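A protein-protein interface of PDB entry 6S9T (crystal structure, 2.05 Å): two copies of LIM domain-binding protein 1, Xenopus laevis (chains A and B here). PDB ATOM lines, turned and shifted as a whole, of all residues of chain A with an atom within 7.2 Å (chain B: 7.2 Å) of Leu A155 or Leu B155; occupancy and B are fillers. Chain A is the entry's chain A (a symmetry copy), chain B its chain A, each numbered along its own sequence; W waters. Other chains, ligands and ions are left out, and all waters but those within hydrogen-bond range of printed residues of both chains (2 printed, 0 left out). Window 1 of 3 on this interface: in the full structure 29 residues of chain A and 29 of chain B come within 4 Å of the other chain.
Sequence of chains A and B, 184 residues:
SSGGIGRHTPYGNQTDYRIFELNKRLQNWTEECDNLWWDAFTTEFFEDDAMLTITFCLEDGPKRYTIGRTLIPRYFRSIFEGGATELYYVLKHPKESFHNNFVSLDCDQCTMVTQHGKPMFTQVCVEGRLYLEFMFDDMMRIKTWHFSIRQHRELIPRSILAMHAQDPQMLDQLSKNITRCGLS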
ATOM      1  N   GLN A 115     -22.002 -14.715   7.730  1.00  0.00           N
ATOM      2  CA  GLN A 115     -21.064 -14.857   6.608  1.00  0.00           C
ATOM      3  C   GLN A 115     -19.882 -13.890   6.843  1.00  0.00           C
ATOM      4  O   GLN A 115     -20.094 -12.804   7.373  1.00  0.00           O
ATOM      5  CB  GLN A 115     -21.790 -14.531   5.316  1.00  0.00           C
ATOM      6  CG  GLN A 115     -20.896 -14.717   4.100  1.00  0.00           C
ATOM      7  CD  GLN A 115     -20.631 -16.197   3.942  1.00  0.00           C
ATOM      8  OE1 GLN A 115     -21.573 -16.975   3.750  1.00  0.00           O
ATOM      9  NE2 GLN A 115     -19.390 -16.602   4.116  1.00  0.00           N
ATOM     10  N   MET A 120     -11.457 -16.481   2.969  1.00  0.00           N
ATOM     11  CA  MET A 120     -11.924 -17.811   3.317  1.00  0.00           C
ATOM     12  C   MET A 120     -13.442 -17.924   3.176  1.00  0.00           C
ATOM     13  O   MET A 120     -13.963 -19.049   3.217  1.00  0.00           O
ATOM     14  CB  MET A 120     -11.525 -18.195   4.742  1.00  0.00           C
ATOM     15  CG  MET A 120     -10.044 -18.129   5.033  1.00  0.00           C
ATOM     16  SD  MET A 120      -8.991 -19.005   3.633  1.00  0.00           S
ATOM     17  CE  MET A 120      -7.107 -18.697   4.160  1.00  0.00           C
ATOM     18  N   PHE A 121     -14.136 -16.782   3.053  1.00  0.00           N
ATOM     19  CA  PHE A 121     -15.591 -16.772   3.002  1.00  0.00           C
ATOM     20  C   PHE A 121     -16.140 -17.715   4.075  1.00  0.00           C
ATOM     21  O   PHE A 121     -17.123 -18.386   3.815  1.00  0.00           O
ATOM     22  CB  PHE A 121     -16.094 -17.143   1.600  1.00  0.00           C
ATOM     23  CG  PHE A 121     -15.623 -16.174   0.555  1.00  0.00           C
ATOM     24  CD1 PHE A 121     -16.297 -14.976   0.353  1.00  0.00           C
ATOM     25  CD2 PHE A 121     -14.419 -16.376  -0.108  1.00  0.00           C
ATOM     26  CE1 PHE A 121     -15.815 -14.030  -0.544  1.00  0.00           C
ATOM     27  CE2 PHE A 121     -13.942 -15.437  -1.017  1.00  0.00           C
ATOM     28  CZ  PHE A 121     -14.640 -14.267  -1.236  1.00  0.00           C
ATOM     29  N   THR A 122     -15.493 -17.781   5.238  1.00  0.00           N
ATOM     30  CA  THR A 122     -15.963 -18.607   6.379  1.00  0.00           C
ATOM     31  C   THR A 122     -17.419 -18.262   6.708  1.00  0.00           C
ATOM     32  O   THR A 122     -17.731 -17.074   6.829  1.00  0.00           O
ATOM     33  CB  THR A 122     -15.102 -18.403   7.619  1.00  0.00           C
ATOM     34  OG1 THR A 122     -13.743 -18.565   7.225  1.00  0.00           O
ATOM     35  CG2 THR A 122     -15.429 -19.387   8.716  1.00  0.00           C
ATOM     36  N   GLN A 123     -18.284 -19.263   6.840  1.00  0.00           N
ATOM     37  CA  GLN A 123     -19.613 -19.088   7.465  1.00  0.00           C
ATOM     38  C   GLN A 123     -19.529 -19.655   8.891  1.00  0.00           C
ATOM     39  O   GLN A 123     -19.122 -20.820   9.045  1.00  0.00           O
ATOM     40  CB  GLN A 123     -20.693 -19.750   6.618  1.00  0.00           C
ATOM     41  CG  GLN A 123     -22.088 -19.646   7.231  1.00  0.00           C
ATOM     42  CD  GLN A 123     -23.188 -20.230   6.382  1.00  0.00           C
ATOM     43  OE1 GLN A 123     -23.460 -19.758   5.282  1.00  0.00           O
ATOM     44  NE2 GLN A 123     -23.818 -21.266   6.893  1.00  0.00           N
ATOM     45  N   VAL A 124     -19.873 -18.861   9.898  1.00  0.00           N
ATOM     46  CA  VAL A 124     -19.909 -19.342  11.305  1.00  0.00           C
ATOM     47  C   VAL A 124     -21.377 -19.564  11.733  1.00  0.00           C
ATOM     48  O   VAL A 124     -22.228 -18.691  11.473  1.00  0.00           O
ATOM     49  CB  VAL A 124     -19.165 -18.380  12.234  1.00  0.00           C
ATOM     50  CG1 VAL A 124     -19.322 -18.746  13.706  1.00  0.00           C
ATOM     51  CG2 VAL A 124     -17.693 -18.275  11.868  1.00  0.00           C
ATOM     52  N   CYS A 125     -21.643 -20.723  12.340  1.00  0.00           N
ATOM     53  CA  CYS A 125     -22.979 -21.154  12.815  1.00  0.00           C
ATOM     54  C   CYS A 125     -22.856 -21.463  14.284  1.00  0.00           C
ATOM     55  O   CYS A 125     -22.238 -22.474  14.629  1.00  0.00           O
ATOM     56  CB  CYS A 125     -23.532 -22.361  12.072  1.00  0.00           C
ATOM     57  SG  CYS A 125     -23.757 -21.925  10.341  1.00  0.00           S
ATOM     58  N   ARG A 153     -20.226 -24.356  14.446  1.00  0.00           N
ATOM     59  CA  ARG A 153     -19.705 -24.956  13.218  1.00  0.00           C
ATOM     60  C   ARG A 153     -19.077 -23.811  12.432  1.00  0.00           C
ATOM     61  O   ARG A 153     -19.655 -22.712  12.421  1.00  0.00           O
ATOM     62  CB  ARG A 153     -20.849 -25.658  12.492  1.00  0.00           C
ATOM     63  CG  ARG A 153     -21.566 -26.726  13.320  1.00  0.00           C
ATOM     64  CD  ARG A 153     -21.111 -28.159  13.070  1.00  0.00           C
ATOM     65  NE  ARG A 153     -21.018 -28.315  11.621  1.00  0.00           N
ATOM     66  CZ  ARG A 153     -21.937 -28.865  10.820  1.00  0.00           C
ATOM     67  NH1 ARG A 153     -23.047 -29.417  11.288  1.00  0.00           N
ATOM     68  NH2 ARG A 153     -21.721 -28.875   9.518  1.00  0.00           N
ATOM     69  N   GLU A 154     -17.932 -24.075  11.823  1.00  0.00           N
ATOM     70  CA  GLU A 154     -17.260 -23.149  10.899  1.00  0.00           C
ATOM     71  C   GLU A 154     -17.267 -23.817   9.516  1.00  0.00           C
ATOM     72  O   GLU A 154     -16.662 -24.911   9.368  1.00  0.00           O
ATOM     73  CB  GLU A 154     -15.870 -22.802  11.441  1.00  0.00           C
ATOM     74  CG  GLU A 154     -15.875 -22.268  12.869  1.00  0.00           C
ATOM     75  CD  GLU A 154     -14.507 -21.867  13.409  1.00  0.00           C
ATOM     76  OE1 GLU A 154     -13.540 -21.787  12.617  1.00  0.00           O
ATOM     77  OE2 GLU A 154     -14.399 -21.641  14.622  1.00  0.00           O
ATOM     78  N   LEU A 155     -17.926 -23.199   8.535  1.00  0.00           N
ATOM     79  CA  LEU A 155     -18.055 -23.791   7.191  1.00  0.00           C
ATOM     80  C   LEU A 155     -17.145 -23.054   6.211  1.00  0.00           C
ATOM     81  O   LEU A 155     -17.070 -21.811   6.281  1.00  0.00           O
ATOM     82  CB  LEU A 155     -19.521 -23.774   6.751  1.00  0.00           C
ATOM     83  CG  LEU A 155     -20.543 -24.208   7.811  1.00  0.00           C
ATOM     84  CD1 LEU A 155     -21.957 -24.271   7.224  1.00  0.00           C
ATOM     85  CD2 LEU A 155     -20.186 -25.561   8.391  1.00  0.00           C
ATOM     86  N   ILE A 156     -16.485 -23.836   5.357  1.00  0.00           N
ATOM     87  CA  ILE A 156     -15.522 -23.449   4.294  1.00  0.00           C
ATOM     88  C   ILE A 156     -16.160 -23.743   2.953  1.00  0.00           C
ATOM     89  O   ILE A 156     -16.611 -24.850   2.744  1.00  0.00           O
ATOM     90  CB  ILE A 156     -14.225 -24.285   4.472  1.00  0.00           C
ATOM     91  CG1 ILE A 156     -13.807 -24.270   5.936  1.00  0.00           C
ATOM     92  CG2 ILE A 156     -13.091 -23.807   3.589  1.00  0.00           C
ATOM     93  CD1 ILE A 156     -13.642 -22.876   6.446  1.00  0.00           C
ATOM     94  N   PRO A 157     -16.194 -22.818   1.988  1.00  0.00           N
ATOM     95  CA  PRO A 157     -16.582 -23.169   0.625  1.00  0.00           C
ATOM     96  C   PRO A 157     -15.640 -24.239   0.062  1.00  0.00           C
ATOM     97  O   PRO A 157     -14.412 -24.185   0.317  1.00  0.00           O
ATOM     98  CB  PRO A 157     -16.381 -21.900  -0.196  1.00  0.00           C
ATOM     99  CG  PRO A 157     -16.315 -20.786   0.838  1.00  0.00           C
ATOM    100  CD  PRO A 157     -15.893 -21.405   2.152  1.00  0.00           C
ATOM    101  N   ARG A 158     -16.194 -25.165  -0.693  1.00  0.00           N
ATOM    102  CA  ARG A 158     -15.409 -26.225  -1.350  1.00  0.00           C
ATOM    103  C   ARG A 158     -14.315 -25.593  -2.207  1.00  0.00           C
ATOM    104  O   ARG A 158     -13.200 -26.095  -2.147  1.00  0.00           O
ATOM    105  CB  ARG A 158     -16.299 -27.131  -2.184  1.00  0.00           C
ATOM    106  CG  ARG A 158     -15.569 -28.390  -2.617  1.00  0.00           C
ATOM    107  CD  ARG A 158     -16.399 -29.204  -3.570  1.00  0.00           C
ATOM    108  NE  ARG A 158     -17.765 -29.451  -3.116  1.00  0.00           N
ATOM    109  CZ  ARG A 158     -18.128 -30.290  -2.136  1.00  0.00           C
ATOM    110  NH1 ARG A 158     -17.231 -30.942  -1.419  1.00  0.00           N
ATOM    111  NH2 ARG A 158     -19.398 -30.451  -1.855  1.00  0.00           N
ATOM    112  N   GLN B 115     -29.270 -27.988   4.305  1.00  0.00           N
ATOM    113  CA  GLN B 115     -28.296 -28.796   5.051  1.00  0.00           C
ATOM    114  C   GLN B 115     -28.459 -30.270   4.614  1.00  0.00           C
ATOM    115  O   GLN B 115     -29.578 -30.695   4.346  1.00  0.00           O
ATOM    116  CB  GLN B 115     -28.555 -28.633   6.536  1.00  0.00           C
ATOM    117  CG  GLN B 115     -27.542 -29.394   7.376  1.00  0.00           C
ATOM    118  CD  GLN B 115     -26.202 -28.711   7.218  1.00  0.00           C
ATOM    119  OE1 GLN B 115     -26.065 -27.533   7.569  1.00  0.00           O
ATOM    120  NE2 GLN B 115     -25.253 -29.395   6.613  1.00  0.00           N
ATOM    121  N   MET B 120     -20.587 -35.775   5.276  1.00  0.00           N
ATOM    122  CA  MET B 120     -19.924 -34.541   4.891  1.00  0.00           C
ATOM    123  C   MET B 120     -20.637 -33.320   5.471  1.00  0.00           C
ATOM    124  O   MET B 120     -20.070 -32.218   5.421  1.00  0.00           O
ATOM    125  CB  MET B 120     -19.843 -34.396   3.370  1.00  0.00           C
ATOM    126  CG  MET B 120     -19.160 -35.537   2.653  1.00  0.00           C
ATOM    127  SD  MET B 120     -17.469 -36.024   3.512  1.00  0.00           S
ATOM    128  CE  MET B 120     -16.821 -37.589   2.486  1.00  0.00           C
ATOM    129  N   PHE B 121     -21.869 -33.505   5.974  1.00  0.00           N
ATOM    130  CA  PHE B 121     -22.669 -32.395   6.469  1.00  0.00           C
ATOM    131  C   PHE B 121     -22.574 -31.227   5.485  1.00  0.00           C
ATOM    132  O   PHE B 121     -22.521 -30.093   5.929  1.00  0.00           O
ATOM    133  CB  PHE B 121     -22.232 -31.991   7.884  1.00  0.00           C
ATOM    134  CG  PHE B 121     -22.398 -33.112   8.868  1.00  0.00           C
ATOM    135  CD1 PHE B 121     -23.636 -33.359   9.447  1.00  0.00           C
ATOM    136  CD2 PHE B 121     -21.370 -34.019   9.091  1.00  0.00           C
ATOM    137  CE1 PHE B 121     -23.824 -34.452  10.287  1.00  0.00           C
ATOM    138  CE2 PHE B 121     -21.552 -35.104   9.942  1.00  0.00           C
ATOM    139  CZ  PHE B 121     -22.777 -35.319  10.541  1.00  0.00           C
ATOM    140  N   THR B 122     -22.520 -31.508   4.184  1.00  0.00           N
ATOM    141  CA  THR B 122     -22.493 -30.463   3.130  1.00  0.00           C
ATOM    142  C   THR B 122     -23.669 -29.500   3.320  1.00  0.00           C
ATOM    143  O   THR B 122     -24.798 -29.972   3.483  1.00  0.00           O
ATOM    144  CB  THR B 122     -22.552 -31.065   1.732  1.00  0.00           C
ATOM    145  OG1 THR B 122     -21.551 -32.075   1.661  1.00  0.00           O
ATOM    146  CG2 THR B 122     -22.310 -30.039   0.652  1.00  0.00           C
ATOM    147  N   GLN B 123     -23.417 -28.195   3.309  1.00  0.00           N
ATOM    148  CA  GLN B 123     -24.482 -27.180   3.155  1.00  0.00           C
ATOM    149  C   GLN B 123     -24.435 -26.679   1.704  1.00  0.00           C
ATOM    150  O   GLN B 123     -23.355 -26.253   1.256  1.00  0.00           O
ATOM    151  CB  GLN B 123     -24.311 -26.067   4.182  1.00  0.00           C
ATOM    152  CG  GLN B 123     -25.354 -24.960   4.049  1.00  0.00           C
ATOM    153  CD  GLN B 123     -25.254 -23.879   5.095  1.00  0.00           C
ATOM    154  OE1 GLN B 123     -25.433 -24.127   6.284  1.00  0.00           O
ATOM    155  NE2 GLN B 123     -24.960 -22.676   4.650  1.00  0.00           N
ATOM    156  N   VAL B 124     -25.548 -26.748   0.984  1.00  0.00           N
ATOM    157  CA  VAL B 124     -25.627 -26.210  -0.400  1.00  0.00           C
ATOM    158  C   VAL B 124     -26.403 -24.874  -0.386  1.00  0.00           C
ATOM    159  O   VAL B 124     -27.471 -24.794   0.252  1.00  0.00           O
ATOM    160  CB  VAL B 124     -26.243 -27.236  -1.354  1.00  0.00           C
ATOM    161  CG1 VAL B 124     -26.498 -26.665  -2.745  1.00  0.00           C
ATOM    162  CG2 VAL B 124     -25.393 -28.495  -1.446  1.00  0.00           C
ATOM    163  N   CYS B 125     -25.841 -23.862  -1.051  1.00  0.00           N
ATOM    164  CA  CYS B 125     -26.397 -22.492  -1.154  1.00  0.00           C
ATOM    165  C   CYS B 125     -26.540 -22.173  -2.619  1.00  0.00           C
ATOM    166  O   CYS B 125     -25.521 -21.974  -3.287  1.00  0.00           O
ATOM    167  CB  CYS B 125     -25.543 -21.434  -0.470  1.00  0.00           C
ATOM    168  SG  CYS B 125     -25.474 -21.793   1.292  1.00  0.00           S
ATOM    169  N   ARG B 153     -22.893 -22.397  -4.018  1.00  0.00           N
ATOM    170  CA  ARG B 153     -21.763 -22.618  -3.116  1.00  0.00           C
ATOM    171  C   ARG B 153     -22.057 -23.928  -2.395  1.00  0.00           C
ATOM    172  O   ARG B 153     -23.224 -24.160  -2.040  1.00  0.00           O
ATOM    173  CB  ARG B 153     -21.633 -21.411  -2.189  1.00  0.00           C
ATOM    174  CG  ARG B 153     -21.460 -20.074  -2.910  1.00  0.00           C
ATOM    175  CD  ARG B 153     -20.023 -19.580  -3.033  1.00  0.00           C
ATOM    176  NE  ARG B 153     -19.407 -19.776  -1.724  1.00  0.00           N
ATOM    177  CZ  ARG B 153     -19.246 -18.849  -0.773  1.00  0.00           C
ATOM    178  NH1 ARG B 153     -19.580 -17.580  -0.957  1.00  0.00           N
ATOM    179  NH2 ARG B 153     -18.720 -19.208   0.383  1.00  0.00           N
ATOM    180  N   GLU B 154     -21.031 -24.744  -2.214  1.00  0.00           N
ATOM    181  CA  GLU B 154     -21.089 -25.973  -1.411  1.00  0.00           C
ATOM    182  C   GLU B 154     -20.153 -25.767  -0.210  1.00  0.00           C
ATOM    183  O   GLU B 154     -18.926 -25.584  -0.424  1.00  0.00           O
ATOM    184  CB  GLU B 154     -20.752 -27.179  -2.293  1.00  0.00           C
ATOM    185  CG  GLU B 154     -21.604 -27.287  -3.552  1.00  0.00           C
ATOM    186  CD  GLU B 154     -21.320 -28.508  -4.417  1.00  0.00           C
ATOM    187  OE1 GLU B 154     -20.601 -29.426  -3.958  1.00  0.00           O
ATOM    188  OE2 GLU B 154     -21.806 -28.547  -5.556  1.00  0.00           O
ATOM    189  N   LEU B 155     -20.695 -25.789   1.007  1.00  0.00           N
ATOM    190  CA  LEU B 155     -19.897 -25.528   2.219  1.00  0.00           C
ATOM    191  C   LEU B 155     -19.661 -26.835   2.973  1.00  0.00           C
ATOM    192  O   LEU B 155     -20.601 -27.648   3.073  1.00  0.00           O
ATOM    193  CB  LEU B 155     -20.591 -24.473   3.085  1.00  0.00           C
ATOM    194  CG  LEU B 155     -21.149 -23.255   2.336  1.00  0.00           C
ATOM    195  CD1 LEU B 155     -21.705 -22.213   3.311  1.00  0.00           C
ATOM    196  CD2 LEU B 155     -20.082 -22.609   1.475  1.00  0.00           C
ATOM    197  N   ILE B 156     -18.428 -26.994   3.454  1.00  0.00           N
ATOM    198  CA  ILE B 156     -17.866 -28.138   4.217  1.00  0.00           C
ATOM    199  C   ILE B 156     -17.583 -27.668   5.627  1.00  0.00           C
ATOM    200  O   ILE B 156     -16.914 -26.669   5.793  1.00  0.00           O
ATOM    201  CB  ILE B 156     -16.554 -28.597   3.525  1.00  0.00           C
ATOM    202  CG1 ILE B 156     -16.783 -28.708   2.023  1.00  0.00           C
ATOM    203  CG2 ILE B 156     -16.024 -29.903   4.079  1.00  0.00           C
ATOM    204  CD1 ILE B 156     -17.925 -29.617   1.706  1.00  0.00           C
ATOM    205  N   PRO B 157     -18.021 -28.358   6.685  1.00  0.00           N
ATOM    206  CA  PRO B 157     -17.547 -28.050   8.032  1.00  0.00           C
ATOM    207  C   PRO B 157     -16.024 -28.204   8.109  1.00  0.00           C
ATOM    208  O   PRO B 157     -15.461 -29.148   7.501  1.00  0.00           O
ATOM    209  CB  PRO B 157     -18.165 -29.112   8.934  1.00  0.00           C
ATOM    210  CG  PRO B 157     -19.305 -29.692   8.113  1.00  0.00           C
ATOM    211  CD  PRO B 157     -18.995 -29.437   6.654  1.00  0.00           C
ATOM    212  N   ARG B 158     -15.385 -27.321   8.847  1.00  0.00           N
ATOM    213  CA  ARG B 158     -13.927 -27.375   9.062  1.00  0.00           C
ATOM    214  C   ARG B 158     -13.546 -28.740   9.628  1.00  0.00           C
ATOM    215  O   ARG B 158     -12.557 -29.283   9.154  1.00  0.00           O
ATOM    216  CB  ARG B 158     -13.466 -26.256   9.980  1.00  0.00           C
ATOM    217  CG  ARG B 158     -11.955 -26.110   9.971  1.00  0.00           C
ATOM    218  CD  ARG B 158     -11.495 -25.113  10.998  1.00  0.00           C
ATOM    219  NE  ARG B 158     -12.202 -23.835  10.953  1.00  0.00           N
ATOM    220  CZ  ARG B 158     -12.057 -22.889  10.015  1.00  0.00           C
ATOM    221  NH1 ARG B 158     -11.274 -23.070   8.967  1.00  0.00           N
ATOM    222  NH2 ARG B 158     -12.724 -21.765  10.116  1.00  0.00           N
HETATM  223  O   HOH W   1     -11.350 -20.444   7.664  1.00  0.00           O
HETATM  224  O   HOH W   2     -18.904 -32.700   0.229  1.00  0.00           O
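The guanidinium group (NH2) of Arg B158 is in salt-bridge range of the side-chain carboxylate (OE1) of Glu A154 (2.6 Å). The backbone carbonyl oxygen (O) of Ile B156 lies within hydrogen-bond range of the backbone NH (N) of Ile A156, at 2.9 Å. The guanidinium group (NH2) of Arg A158 lies within salt-bridge range of the side-chain carboxylate (OE1) of Glu B154 (2.6 Å). NE2 of Gln A123 lies close to NE2 of Gln B123 (2.9 Å).
The side-chain amide nitrogen of Gln A123 lies within hydrogen-bond range of the side-chain sulfur of Cys A125 (3.5 Å). NE2 of Gln B115 sits at hydrogen-bond distance from O of Thr B122, at 3.2 Å. The side-chain amide nitrogen of Gln A115 lies within hydrogen-bond range of the backbone carbonyl oxygen of Phe A121. O of Cys A125 sits at hydrogen-bond distance from N of Arg A153. The backbone NH of Arg B153 lies within hydrogen-bond range of the backbone carbonyl oxygen of Cys B125 (2.8 Å). NE2 of Gln B115 lies within hydrogen-bond range of O of Phe B121, at 2.9 Å.
Among the printed residues, pairs that only touch across the chains: Phe A121 with Arg B153, Thr A122 with Arg B158, Gln A123 with Leu B155, Arg A153 with Phe B121, Arg A153 with Pro B157, Glu A154 with Ile B156, Glu A154 with Pro B157, Leu A155 with Gln B123, Leu A155 with Leu B155, Leu A155 with Ile B156, Leu A155 with Pro B157, Ile A156 with Glu B154, Ile A156 with Leu B155, Ile A156 with Arg B158, Pro A157 with Arg B153, Pro A157 with Glu B154, Pro A157 with Leu B155, Arg A158 with Thr B122 and Arg A158 with Ile B156.
Of the printed residues of chain B, Arg A153 touches Phe B121 (3.6 Å) and Pro B157 (2.9 Å). Printed residues of chain B within 4 Å of Glu A154: Ile B156, Pro B157 and Arg B158. Leu A155 touches four residues of chain B. Printed residues of chain A within 4 Å of Gln B123: Gln A123 and Leu A155. Of chain A, only Gln A123, Leu A155, Ile A156 and Pro A157 come within 4 Å of Leu B155. The nearest residue of chain B that does not touch Leu A155 is Arg B158 (4.7 Å). The nearest residue of chain A that does not touch Leu B155 is Arg A158 (4.7 Å). The nearest printed residue of chain A that does not touch Glu B154 is Leu A155 (7.3 Å).
Hydrophobic or aromatic side chains of chain A within 4 Å of the printed part of chain B: Phe A121, Leu A155, Ile A156 and Pro A157. Among the printed residues, 23 pairs touch across the chains. Among the printed residues, Asp or Glu carboxylates within 4 Å of a Lys or Arg side-chain nitrogen of the other chain: Glu A154 with Arg B158 and Arg A158 with Glu B154.
Thr A122 touches Arg B158, and with the chains exchanged Arg A158 touches Thr B122. Gln A123 touches its own counterpart, Gln B123. Gln A123 touches Leu B155, and with the chains exchanged Leu A155 touches Gln B123. Glu A154 touches Ile B156, and with the chains exchanged Ile A156 touches Glu B154.
Water W1 bridges the guanidinium group of Arg B158 and the side-chain hydroxyl of Thr A122. Water W2 bridges the guanidinium group (NH1) of Arg A158 and the side-chain hydroxyl (OG1) of Thr B122.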
